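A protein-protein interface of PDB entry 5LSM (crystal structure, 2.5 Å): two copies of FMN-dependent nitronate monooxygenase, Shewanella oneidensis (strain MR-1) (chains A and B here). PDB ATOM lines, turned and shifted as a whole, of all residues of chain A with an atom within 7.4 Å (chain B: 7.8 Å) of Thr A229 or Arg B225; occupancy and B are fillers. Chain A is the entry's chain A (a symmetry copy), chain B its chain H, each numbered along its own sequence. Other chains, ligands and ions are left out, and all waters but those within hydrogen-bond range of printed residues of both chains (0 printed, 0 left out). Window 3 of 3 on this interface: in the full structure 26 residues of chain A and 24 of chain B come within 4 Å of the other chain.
Of chain B, only Thr B222, Arg B225 and Thr B229 come within 4 Å of Thr A229.
Of the printed residues of chain A, Arg B225 touches Thr A229.
No residue of chain A comes within 4 Å of Val B224.
Of the printed residues of chain B, Ala A226 touches Ala B226 (3.9 Å), Thr B229 (3.7 Å) and Met B230 (3.8 Å).
Printed residues of chain A within 4 Å of Ala B226: Ala A226 (3.9 Å) and Met A230 (3.7 Å).
Ile B218 touches none of the printed residues of chain A.
The nearest residue of chain B that does not touch Thr A229 is Ala B226 (4.1 Å).
The nearest residue of chain A that does not touch Arg B225 is Met A230 (5.2 Å).
The nearest printed residue of chain B that does not touch Met A230 is Arg B225 (5.2 Å).
NH2 of Arg B225 is in hydrogen-bond range of O of Thr A229.
Thr B223 touches Phe A198 (O to CZ, 3.6 Å).
Met B230 touches Thr A222.
CE of Met B230 touches CG2 of Thr A223, at 3.2 Å.
Thr B229 touches Arg A225.
Thr B229 touches Ala A226 (CG2 to N, 3.7 Å).
CB of Ala A226 touches SD of Met B230 (3.8 Å).
O of Thr A229 touches CG2 of Thr B222 (3.7 Å).
OG1 of Thr A229 touches OG1 of Thr B229, 3.8 Å away.
CA of Met A230 touches CG2 of Thr B222, at 3.6 Å.
Met A230 touches Thr B223 (CE to CG2, 3.3 Å).
The side-chain carboxylate of Asp B220 sits close to the backbone NH of Thr B222 (3.3 Å).
The side-chain hydroxyl (OG1) of Thr B223 is in hydrogen-bond range of the side-chain carboxylate (OD1) of Asp B220, at 2.7 Å.
OG1 of Thr B229 lies within hydrogen-bond range of O of Arg B225 (3.1 Å).
The side-chain hydroxyl of Thr A229 sits at hydrogen-bond distance from the backbone carbonyl oxygen of Arg A225 (2.7 Å).
Thr A222 touches Met B230, and with the chains exchanged Met A230 touches Thr B222.
Arg A225 touches Thr B229, and with the chains exchanged Thr A229 touches Arg B225.
Ala A226 touches its own counterpart, Ala B226.
Thr B229 touches its own counterpart, Thr A229.
Positions printed for both chains: 222, 223, 224, 225, 226, 227, 228, 229, 230, 231 and 232.
Of the 16 printed residues of chain B, 6 touch a printed residue of chain A.
Printed residues of chain A that touch a printed residue of chain B: Phe A198, Thr A222, Thr A223, Arg A225, Ala A226, Thr A229 and Met A230.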
ATOM      1  N   PHE A 198       5.901 -37.496  14.420  1.00  0.00           N
ATOM      2  CA  PHE A 198       6.237 -36.092  14.261  1.00  0.00           C
ATOM      3  C   PHE A 198       6.798 -35.807  12.883  1.00  0.00           C
ATOM      4  O   PHE A 198       6.681 -34.696  12.378  1.00  0.00           O
ATOM      5  CB  PHE A 198       7.266 -35.672  15.314  1.00  0.00           C
ATOM      6  CG  PHE A 198       7.233 -34.223  15.635  1.00  0.00           C
ATOM      7  CD1 PHE A 198       6.169 -33.685  16.359  1.00  0.00           C
ATOM      8  CD2 PHE A 198       8.262 -33.390  15.241  1.00  0.00           C
ATOM      9  CE1 PHE A 198       6.132 -32.339  16.653  1.00  0.00           C
ATOM     10  CE2 PHE A 198       8.235 -32.047  15.553  1.00  0.00           C
ATOM     11  CZ  PHE A 198       7.163 -31.518  16.241  1.00  0.00           C
ATOM     12  N   LEU A 201       3.814 -37.702   9.690  1.00  0.00           N
ATOM     13  CA  LEU A 201       2.599 -36.945   9.435  1.00  0.00           C
ATOM     14  C   LEU A 201       2.787 -35.809   8.423  1.00  0.00           C
ATOM     15  O   LEU A 201       2.135 -35.819   7.373  1.00  0.00           O
ATOM     16  CB  LEU A 201       2.027 -36.409  10.741  1.00  0.00           C
ATOM     17  CG  LEU A 201       0.653 -35.765  10.652  1.00  0.00           C
ATOM     18  CD1 LEU A 201      -0.351 -36.791  10.144  1.00  0.00           C
ATOM     19  CD2 LEU A 201       0.233 -35.231  12.027  1.00  0.00           C
ATOM     20  N   ILE A 205       1.418 -35.686   4.495  1.00  0.00           N
ATOM     21  CA  ILE A 205       0.477 -34.635   4.081  1.00  0.00           C
ATOM     22  C   ILE A 205       1.045 -33.849   2.895  1.00  0.00           C
ATOM     23  O   ILE A 205       0.310 -33.490   1.989  1.00  0.00           O
ATOM     24  CB  ILE A 205       0.146 -33.663   5.245  1.00  0.00           C
ATOM     25  CG1 ILE A 205      -0.838 -34.306   6.220  1.00  0.00           C
ATOM     26  CG2 ILE A 205      -0.431 -32.342   4.735  1.00  0.00           C
ATOM     27  CD1 ILE A 205      -0.786 -33.689   7.602  1.00  0.00           C
ATOM     28  N   THR A 222      -4.046 -32.000  24.280  1.00  0.00           N
ATOM     29  CA  THR A 222      -2.846 -31.365  23.770  1.00  0.00           C
ATOM     30  C   THR A 222      -2.312 -32.084  22.549  1.00  0.00           C
ATOM     31  O   THR A 222      -1.971 -31.452  21.566  1.00  0.00           O
ATOM     32  CB  THR A 222      -1.750 -31.327  24.840  1.00  0.00           C
ATOM     33  OG1 THR A 222      -2.111 -30.364  25.820  1.00  0.00           O
ATOM     34  CG2 THR A 222      -0.408 -30.944  24.251  1.00  0.00           C
ATOM     35  N   THR A 223      -2.212 -33.405  22.620  1.00  0.00           N
ATOM     36  CA  THR A 223      -1.607 -34.151  21.528  1.00  0.00           C
ATOM     37  C   THR A 223      -2.524 -34.172  20.303  1.00  0.00           C
ATOM     38  O   THR A 223      -2.043 -34.126  19.157  1.00  0.00           O
ATOM     39  CB  THR A 223      -1.207 -35.594  21.927  1.00  0.00           C
ATOM     40  OG1 THR A 223      -2.215 -36.172  22.748  1.00  0.00           O
ATOM     41  CG2 THR A 223       0.148 -35.616  22.672  1.00  0.00           C
ATOM     42  N   VAL A 224      -3.832 -34.192  20.534  1.00  0.00           N
ATOM     43  CA  VAL A 224      -4.789 -34.046  19.432  1.00  0.00           C
ATOM     44  C   VAL A 224      -4.512 -32.711  18.746  1.00  0.00           C
ATOM     45  O   VAL A 224      -4.411 -32.647  17.510  1.00  0.00           O
ATOM     46  CB  VAL A 224      -6.257 -34.150  19.931  1.00  0.00           C
ATOM     47  CG1 VAL A 224      -7.259 -33.791  18.845  1.00  0.00           C
ATOM     48  CG2 VAL A 224      -6.542 -35.561  20.429  1.00  0.00           C
ATOM     49  N   ARG A 225      -4.242 -31.686  19.557  1.00  0.00           N
ATOM     50  CA  ARG A 225      -4.007 -30.326  19.038  1.00  0.00           C
ATOM     51  C   ARG A 225      -2.741 -30.263  18.184  1.00  0.00           C
ATOM     52  O   ARG A 225      -2.771 -29.748  17.070  1.00  0.00           O
ATOM     53  CB  ARG A 225      -3.932 -29.274  20.173  1.00  0.00           C
ATOM     54  CG  ARG A 225      -3.886 -27.830  19.665  1.00  0.00           C
ATOM     55  CD  ARG A 225      -3.919 -26.776  20.774  1.00  0.00           C
ATOM     56  NE  ARG A 225      -3.725 -25.421  20.231  1.00  0.00           N
ATOM     57  CZ  ARG A 225      -4.639 -24.703  19.558  1.00  0.00           C
ATOM     58  NH1 ARG A 225      -5.883 -25.149  19.385  1.00  0.00           N
ATOM     59  NH2 ARG A 225      -4.303 -23.519  19.056  1.00  0.00           N
ATOM     60  N   ALA A 226      -1.636 -30.769  18.725  1.00  0.00           N
ATOM     61  CA  ALA A 226      -0.386 -30.869  17.968  1.00  0.00           C
ATOM     62  C   ALA A 226      -0.583 -31.567  16.634  1.00  0.00           C
ATOM     63  O   ALA A 226      -0.021 -31.146  15.646  1.00  0.00           O
ATOM     64  CB  ALA A 226       0.663 -31.606  18.781  1.00  0.00           C
ATOM     65  N   ALA A 227      -1.376 -32.638  16.610  1.00  0.00           N
ATOM     66  CA  ALA A 227      -1.629 -33.375  15.361  1.00  0.00           C
ATOM     67  C   ALA A 227      -2.331 -32.511  14.334  1.00  0.00           C
ATOM     68  O   ALA A 227      -1.902 -32.444  13.197  1.00  0.00           O
ATOM     69  CB  ALA A 227      -2.437 -34.644  15.616  1.00  0.00           C
ATOM     70  N   MET A 228      -3.389 -31.823  14.752  1.00  0.00           N
ATOM     71  CA  MET A 228      -4.211 -31.031  13.843  1.00  0.00           C
ATOM     72  C   MET A 228      -3.439 -29.806  13.343  1.00  0.00           C
ATOM     73  O   MET A 228      -3.478 -29.471  12.158  1.00  0.00           O
ATOM     74  CB  MET A 228      -5.487 -30.579  14.554  1.00  0.00           C
ATOM     75  CG  MET A 228      -6.387 -31.700  15.045  1.00  0.00           C
ATOM     76  SD  MET A 228      -6.973 -32.717  13.692  1.00  0.00           S
ATOM     77  CE  MET A 228      -8.144 -33.736  14.573  1.00  0.00           C
ATOM     78  N   THR A 229      -2.725 -29.156  14.255  1.00  0.00           N
ATOM     79  CA  THR A 229      -1.755 -28.101  13.925  1.00  0.00           C
ATOM     80  C   THR A 229      -0.854 -28.437  12.738  1.00  0.00           C
ATOM     81  O   THR A 229      -0.478 -27.560  11.982  1.00  0.00           O
ATOM     82  CB  THR A 229      -0.844 -27.808  15.133  1.00  0.00           C
ATOM     83  OG1 THR A 229      -1.641 -27.391  16.245  1.00  0.00           O
ATOM     84  CG2 THR A 229       0.132 -26.727  14.815  1.00  0.00           C
ATOM     85  N   MET A 230      -0.424 -29.686  12.652  1.00  0.00           N
ATOM     86  CA  MET A 230       0.433 -30.133  11.563  1.00  0.00           C
ATOM     87  C   MET A 230      -0.313 -30.320  10.255  1.00  0.00           C
ATOM     88  O   MET A 230       0.320 -30.565   9.239  1.00  0.00           O
ATOM     89  CB  MET A 230       1.093 -31.465  11.917  1.00  0.00           C
ATOM     90  CG  MET A 230       1.888 -31.449  13.211  1.00  0.00           C
ATOM     91  SD  MET A 230       3.500 -32.211  13.028  1.00  0.00           S
ATOM     92  CE  MET A 230       4.187 -31.121  11.794  1.00  0.00           C
ATOM     93  N   GLY A 231      -1.645 -30.348  10.305  1.00  0.00           N
ATOM     94  CA  GLY A 231      -2.472 -30.476   9.093  1.00  0.00           C
ATOM     95  C   GLY A 231      -3.194 -31.811   8.974  1.00  0.00           C
ATOM     96  O   GLY A 231      -3.706 -32.139   7.922  1.00  0.00           O
ATOM     97  N   ALA A 232      -3.248 -32.587  10.045  1.00  0.00           N
ATOM     98  CA  ALA A 232      -4.097 -33.787  10.048  1.00  0.00           C
ATOM     99  C   ALA A 232      -5.581 -33.408   9.916  1.00  0.00           C
ATOM    100  O   ALA A 232      -6.016 -32.428  10.499  1.00  0.00           O
ATOM    101  CB  ALA A 232      -3.878 -34.585  11.330  1.00  0.00           C
ATOM    102  N   LEU A 347      -9.706 -27.660  20.195  1.00  0.00           N
ATOM    103  CA  LEU A 347      -9.975 -27.358  18.772  1.00  0.00           C
ATOM    104  C   LEU A 347     -10.992 -26.236  18.575  1.00  0.00           C
ATOM    105  O   LEU A 347     -11.841 -26.004  19.438  1.00  0.00           O
ATOM    106  CB  LEU A 347     -10.471 -28.610  18.049  1.00  0.00           C
ATOM    107  CG  LEU A 347      -9.557 -29.819  18.176  1.00  0.00           C
ATOM    108  CD1 LEU A 347     -10.109 -30.980  17.363  1.00  0.00           C
ATOM    109  CD2 LEU A 347      -8.145 -29.446  17.738  1.00  0.00           C
ATOM    110  N   ILE B 218      12.124 -30.905  14.148  1.00  0.00           N
ATOM    111  CA  ILE B 218      11.722 -29.505  14.025  1.00  0.00           C
ATOM    112  C   ILE B 218      12.486 -28.870  12.857  1.00  0.00           C
ATOM    113  O   ILE B 218      13.711 -28.730  12.900  1.00  0.00           O
ATOM    114  CB  ILE B 218      11.920 -28.723  15.349  1.00  0.00           C
ATOM    115  N   ASP B 220      10.610 -26.527  10.319  1.00  0.00           N
ATOM    116  CA  ASP B 220       9.811 -25.491   9.657  1.00  0.00           C
ATOM    117  C   ASP B 220       8.770 -24.906  10.632  1.00  0.00           C
ATOM    118  O   ASP B 220       8.619 -25.391  11.776  1.00  0.00           O
ATOM    119  CB  ASP B 220       9.120 -26.043   8.392  1.00  0.00           C
ATOM    120  CG  ASP B 220       8.084 -27.147   8.692  1.00  0.00           C
ATOM    121  OD1 ASP B 220       7.625 -27.303   9.847  1.00  0.00           O
ATOM    122  OD2 ASP B 220       7.688 -27.850   7.740  1.00  0.00           O
ATOM    123  N   ALA B 221       8.031 -23.896  10.161  1.00  0.00           N
ATOM    124  CA  ALA B 221       7.120 -23.120  11.008  1.00  0.00           C
ATOM    125  C   ALA B 221       6.064 -23.995  11.651  1.00  0.00           C
ATOM    126  O   ALA B 221       5.738 -23.811  12.813  1.00  0.00           O
ATOM    127  CB  ALA B 221       6.455 -22.006  10.204  1.00  0.00           C
ATOM    128  N   THR B 222       5.558 -24.961  10.889  1.00  0.00           N
ATOM    129  CA  THR B 222       4.449 -25.807  11.308  1.00  0.00           C
ATOM    130  C   THR B 222       4.896 -26.724  12.436  1.00  0.00           C
ATOM    131  O   THR B 222       4.200 -26.861  13.443  1.00  0.00           O
ATOM    132  CB  THR B 222       3.959 -26.684  10.132  1.00  0.00           C
ATOM    133  OG1 THR B 222       3.352 -25.859   9.132  1.00  0.00           O
ATOM    134  CG2 THR B 222       2.947 -27.729  10.594  1.00  0.00           C
ATOM    135  N   THR B 223       6.037 -27.388  12.235  1.00  0.00           N
ATOM    136  CA  THR B 223       6.572 -28.309  13.222  1.00  0.00           C
ATOM    137  C   THR B 223       6.992 -27.552  14.475  1.00  0.00           C
ATOM    138  O   THR B 223       6.772 -28.040  15.594  1.00  0.00           O
ATOM    139  CB  THR B 223       7.772 -29.135  12.679  1.00  0.00           C
ATOM    140  OG1 THR B 223       8.726 -28.279  12.067  1.00  0.00           O
ATOM    141  CG2 THR B 223       7.322 -30.144  11.653  1.00  0.00           C
ATOM    142  N   VAL B 224       7.547 -26.351  14.301  1.00  0.00           N
ATOM    143  CA  VAL B 224       7.898 -25.502  15.467  1.00  0.00           C
ATOM    144  C   VAL B 224       6.624 -25.214  16.244  1.00  0.00           C
ATOM    145  O   VAL B 224       6.559 -25.398  17.468  1.00  0.00           O
ATOM    146  CB  VAL B 224       8.606 -24.158  15.072  1.00  0.00           C
ATOM    147  N   ARG B 225       5.579 -24.883  15.503  1.00  0.00           N
ATOM    148  CA  ARG B 225       4.293 -24.566  16.095  1.00  0.00           C
ATOM    149  C   ARG B 225       3.781 -25.772  16.835  1.00  0.00           C
ATOM    150  O   ARG B 225       3.263 -25.643  17.940  1.00  0.00           O
ATOM    151  CB  ARG B 225       3.279 -24.127  15.024  1.00  0.00           C
ATOM    152  CG  ARG B 225       1.978 -23.565  15.591  1.00  0.00           C
ATOM    153  CD  ARG B 225       1.211 -22.733  14.561  1.00  0.00           C
ATOM    154  NE  ARG B 225       0.087 -23.457  13.946  1.00  0.00           N
ATOM    155  CZ  ARG B 225       0.062 -23.954  12.701  1.00  0.00           C
ATOM    156  NH1 ARG B 225       1.116 -23.858  11.889  1.00  0.00           N
ATOM    157  NH2 ARG B 225      -1.033 -24.572  12.266  1.00  0.00           N
ATOM    158  N   ALA B 226       3.949 -26.951  16.239  1.00  0.00           N
ATOM    159  CA  ALA B 226       3.398 -28.168  16.823  1.00  0.00           C
ATOM    160  C   ALA B 226       4.123 -28.539  18.111  1.00  0.00           C
ATOM    161  O   ALA B 226       3.505 -28.993  19.052  1.00  0.00           O
ATOM    162  CB  ALA B 226       3.430 -29.321  15.826  1.00  0.00           C
ATOM    163  N   ALA B 227       5.426 -28.295  18.165  1.00  0.00           N
ATOM    164  CA  ALA B 227       6.186 -28.521  19.387  1.00  0.00           C
ATOM    165  C   ALA B 227       5.846 -27.510  20.481  1.00  0.00           C
ATOM    166  O   ALA B 227       5.767 -27.863  21.656  1.00  0.00           O
ATOM    167  CB  ALA B 227       7.676 -28.507  19.089  1.00  0.00           C
ATOM    168  N   MET B 228       5.673 -26.249  20.120  1.00  0.00           N
ATOM    169  CA  MET B 228       5.317 -25.245  21.135  1.00  0.00           C
ATOM    170  C   MET B 228       3.924 -25.523  21.679  1.00  0.00           C
ATOM    171  O   MET B 228       3.682 -25.366  22.874  1.00  0.00           O
ATOM    172  CB  MET B 228       5.389 -23.819  20.576  1.00  0.00           C
ATOM    173  CG  MET B 228       6.743 -23.429  19.974  1.00  0.00           C
ATOM    174  SD  MET B 228       8.141 -23.346  21.124  1.00  0.00           S
ATOM    175  CE  MET B 228       7.602 -22.051  22.243  1.00  0.00           C
ATOM    176  N   THR B 229       3.035 -26.011  20.814  1.00  0.00           N
ATOM    177  CA  THR B 229       1.659 -26.351  21.206  1.00  0.00           C
ATOM    178  C   THR B 229       1.677 -27.293  22.394  1.00  0.00           C
ATOM    179  O   THR B 229       0.947 -27.095  23.355  1.00  0.00           O
ATOM    180  CB  THR B 229       0.898 -27.026  20.047  1.00  0.00           C
ATOM    181  OG1 THR B 229       0.396 -26.028  19.170  1.00  0.00           O
ATOM    182  CG2 THR B 229      -0.258 -27.843  20.544  1.00  0.00           C
ATOM    183  N   MET B 230       2.523 -28.316  22.304  1.00  0.00           N
ATOM    184  CA  MET B 230       2.679 -29.329  23.354  1.00  0.00           C
ATOM    185  C   MET B 230       3.327 -28.788  24.619  1.00  0.00           C
ATOM    186  O   MET B 230       3.511 -29.516  25.583  1.00  0.00           O
ATOM    187  CB  MET B 230       3.537 -30.479  22.836  1.00  0.00           C
ATOM    188  CG  MET B 230       2.753 -31.732  22.526  1.00  0.00           C
ATOM    189  SD  MET B 230       3.491 -32.595  21.155  1.00  0.00           S
ATOM    190  CE  MET B 230       2.525 -34.091  21.201  1.00  0.00           C
ATOM    191  N   GLY B 231       3.792 -27.552  24.571  1.00  0.00           N
ATOM    192  CA  GLY B 231       4.316 -26.907  25.750  1.00  0.00           C
ATOM    193  C   GLY B 231       5.826 -26.848  25.813  1.00  0.00           C
ATOM    194  O   GLY B 231       6.374 -26.591  26.875  1.00  0.00           O
ATOM    195  N   ALA B 232       6.509 -27.032  24.685  1.00  0.00           N
ATOM    196  CA  ALA B 232       7.951 -26.760  24.652  1.00  0.00           C
ATOM    197  C   ALA B 232       8.186 -25.301  24.976  1.00  0.00           C
ATOM    198  O   ALA B 232       7.414 -24.467  24.585  1.00  0.00           O
ATOM    199  CB  ALA B 232       8.550 -27.097  23.292  1.00  0.00           C
ATOM    200  N   VAL B 235      12.700 -24.680  20.830  1.00  0.00           N
ATOM    201  CA  VAL B 235      13.002 -25.779  19.911  1.00  0.00           C
ATOM    202  C   VAL B 235      14.472 -25.758  19.516  1.00  0.00           C
ATOM    203  O   VAL B 235      15.078 -24.698  19.472  1.00  0.00           O
ATOM    204  CB  VAL B 235      12.112 -25.754  18.645  1.00  0.00           C
ATOM    205  CG1 VAL B 235      10.647 -25.894  19.036  1.00  0.00           C
ATOM    206  CG2 VAL B 235      12.327 -24.480  17.830  1.00  0.00           C
ATOM    207  N   PHE B 343      11.116 -19.738  10.932  1.00  0.00           N
ATOM    208  CA  PHE B 343      10.574 -20.553  12.014  1.00  0.00           C
ATOM    209  C   PHE B 343       9.704 -19.720  12.941  1.00  0.00           C
ATOM    210  O   PHE B 343       9.005 -20.301  13.750  1.00  0.00           O
ATOM    211  CB  PHE B 343      11.688 -21.202  12.822  1.00  0.00           C
ATOM    212  CG  PHE B 343      12.642 -22.017  12.006  1.00  0.00           C
ATOM    213  CD1 PHE B 343      12.202 -22.750  10.915  1.00  0.00           C
ATOM    214  CD2 PHE B 343      13.982 -22.116  12.387  1.00  0.00           C
ATOM    215  CE1 PHE B 343      13.080 -23.546  10.196  1.00  0.00           C
ATOM    216  CE2 PHE B 343      14.866 -22.905  11.668  1.00  0.00           C
ATOM    217  CZ  PHE B 343      14.416 -23.619  10.568  1.00  0.00           C
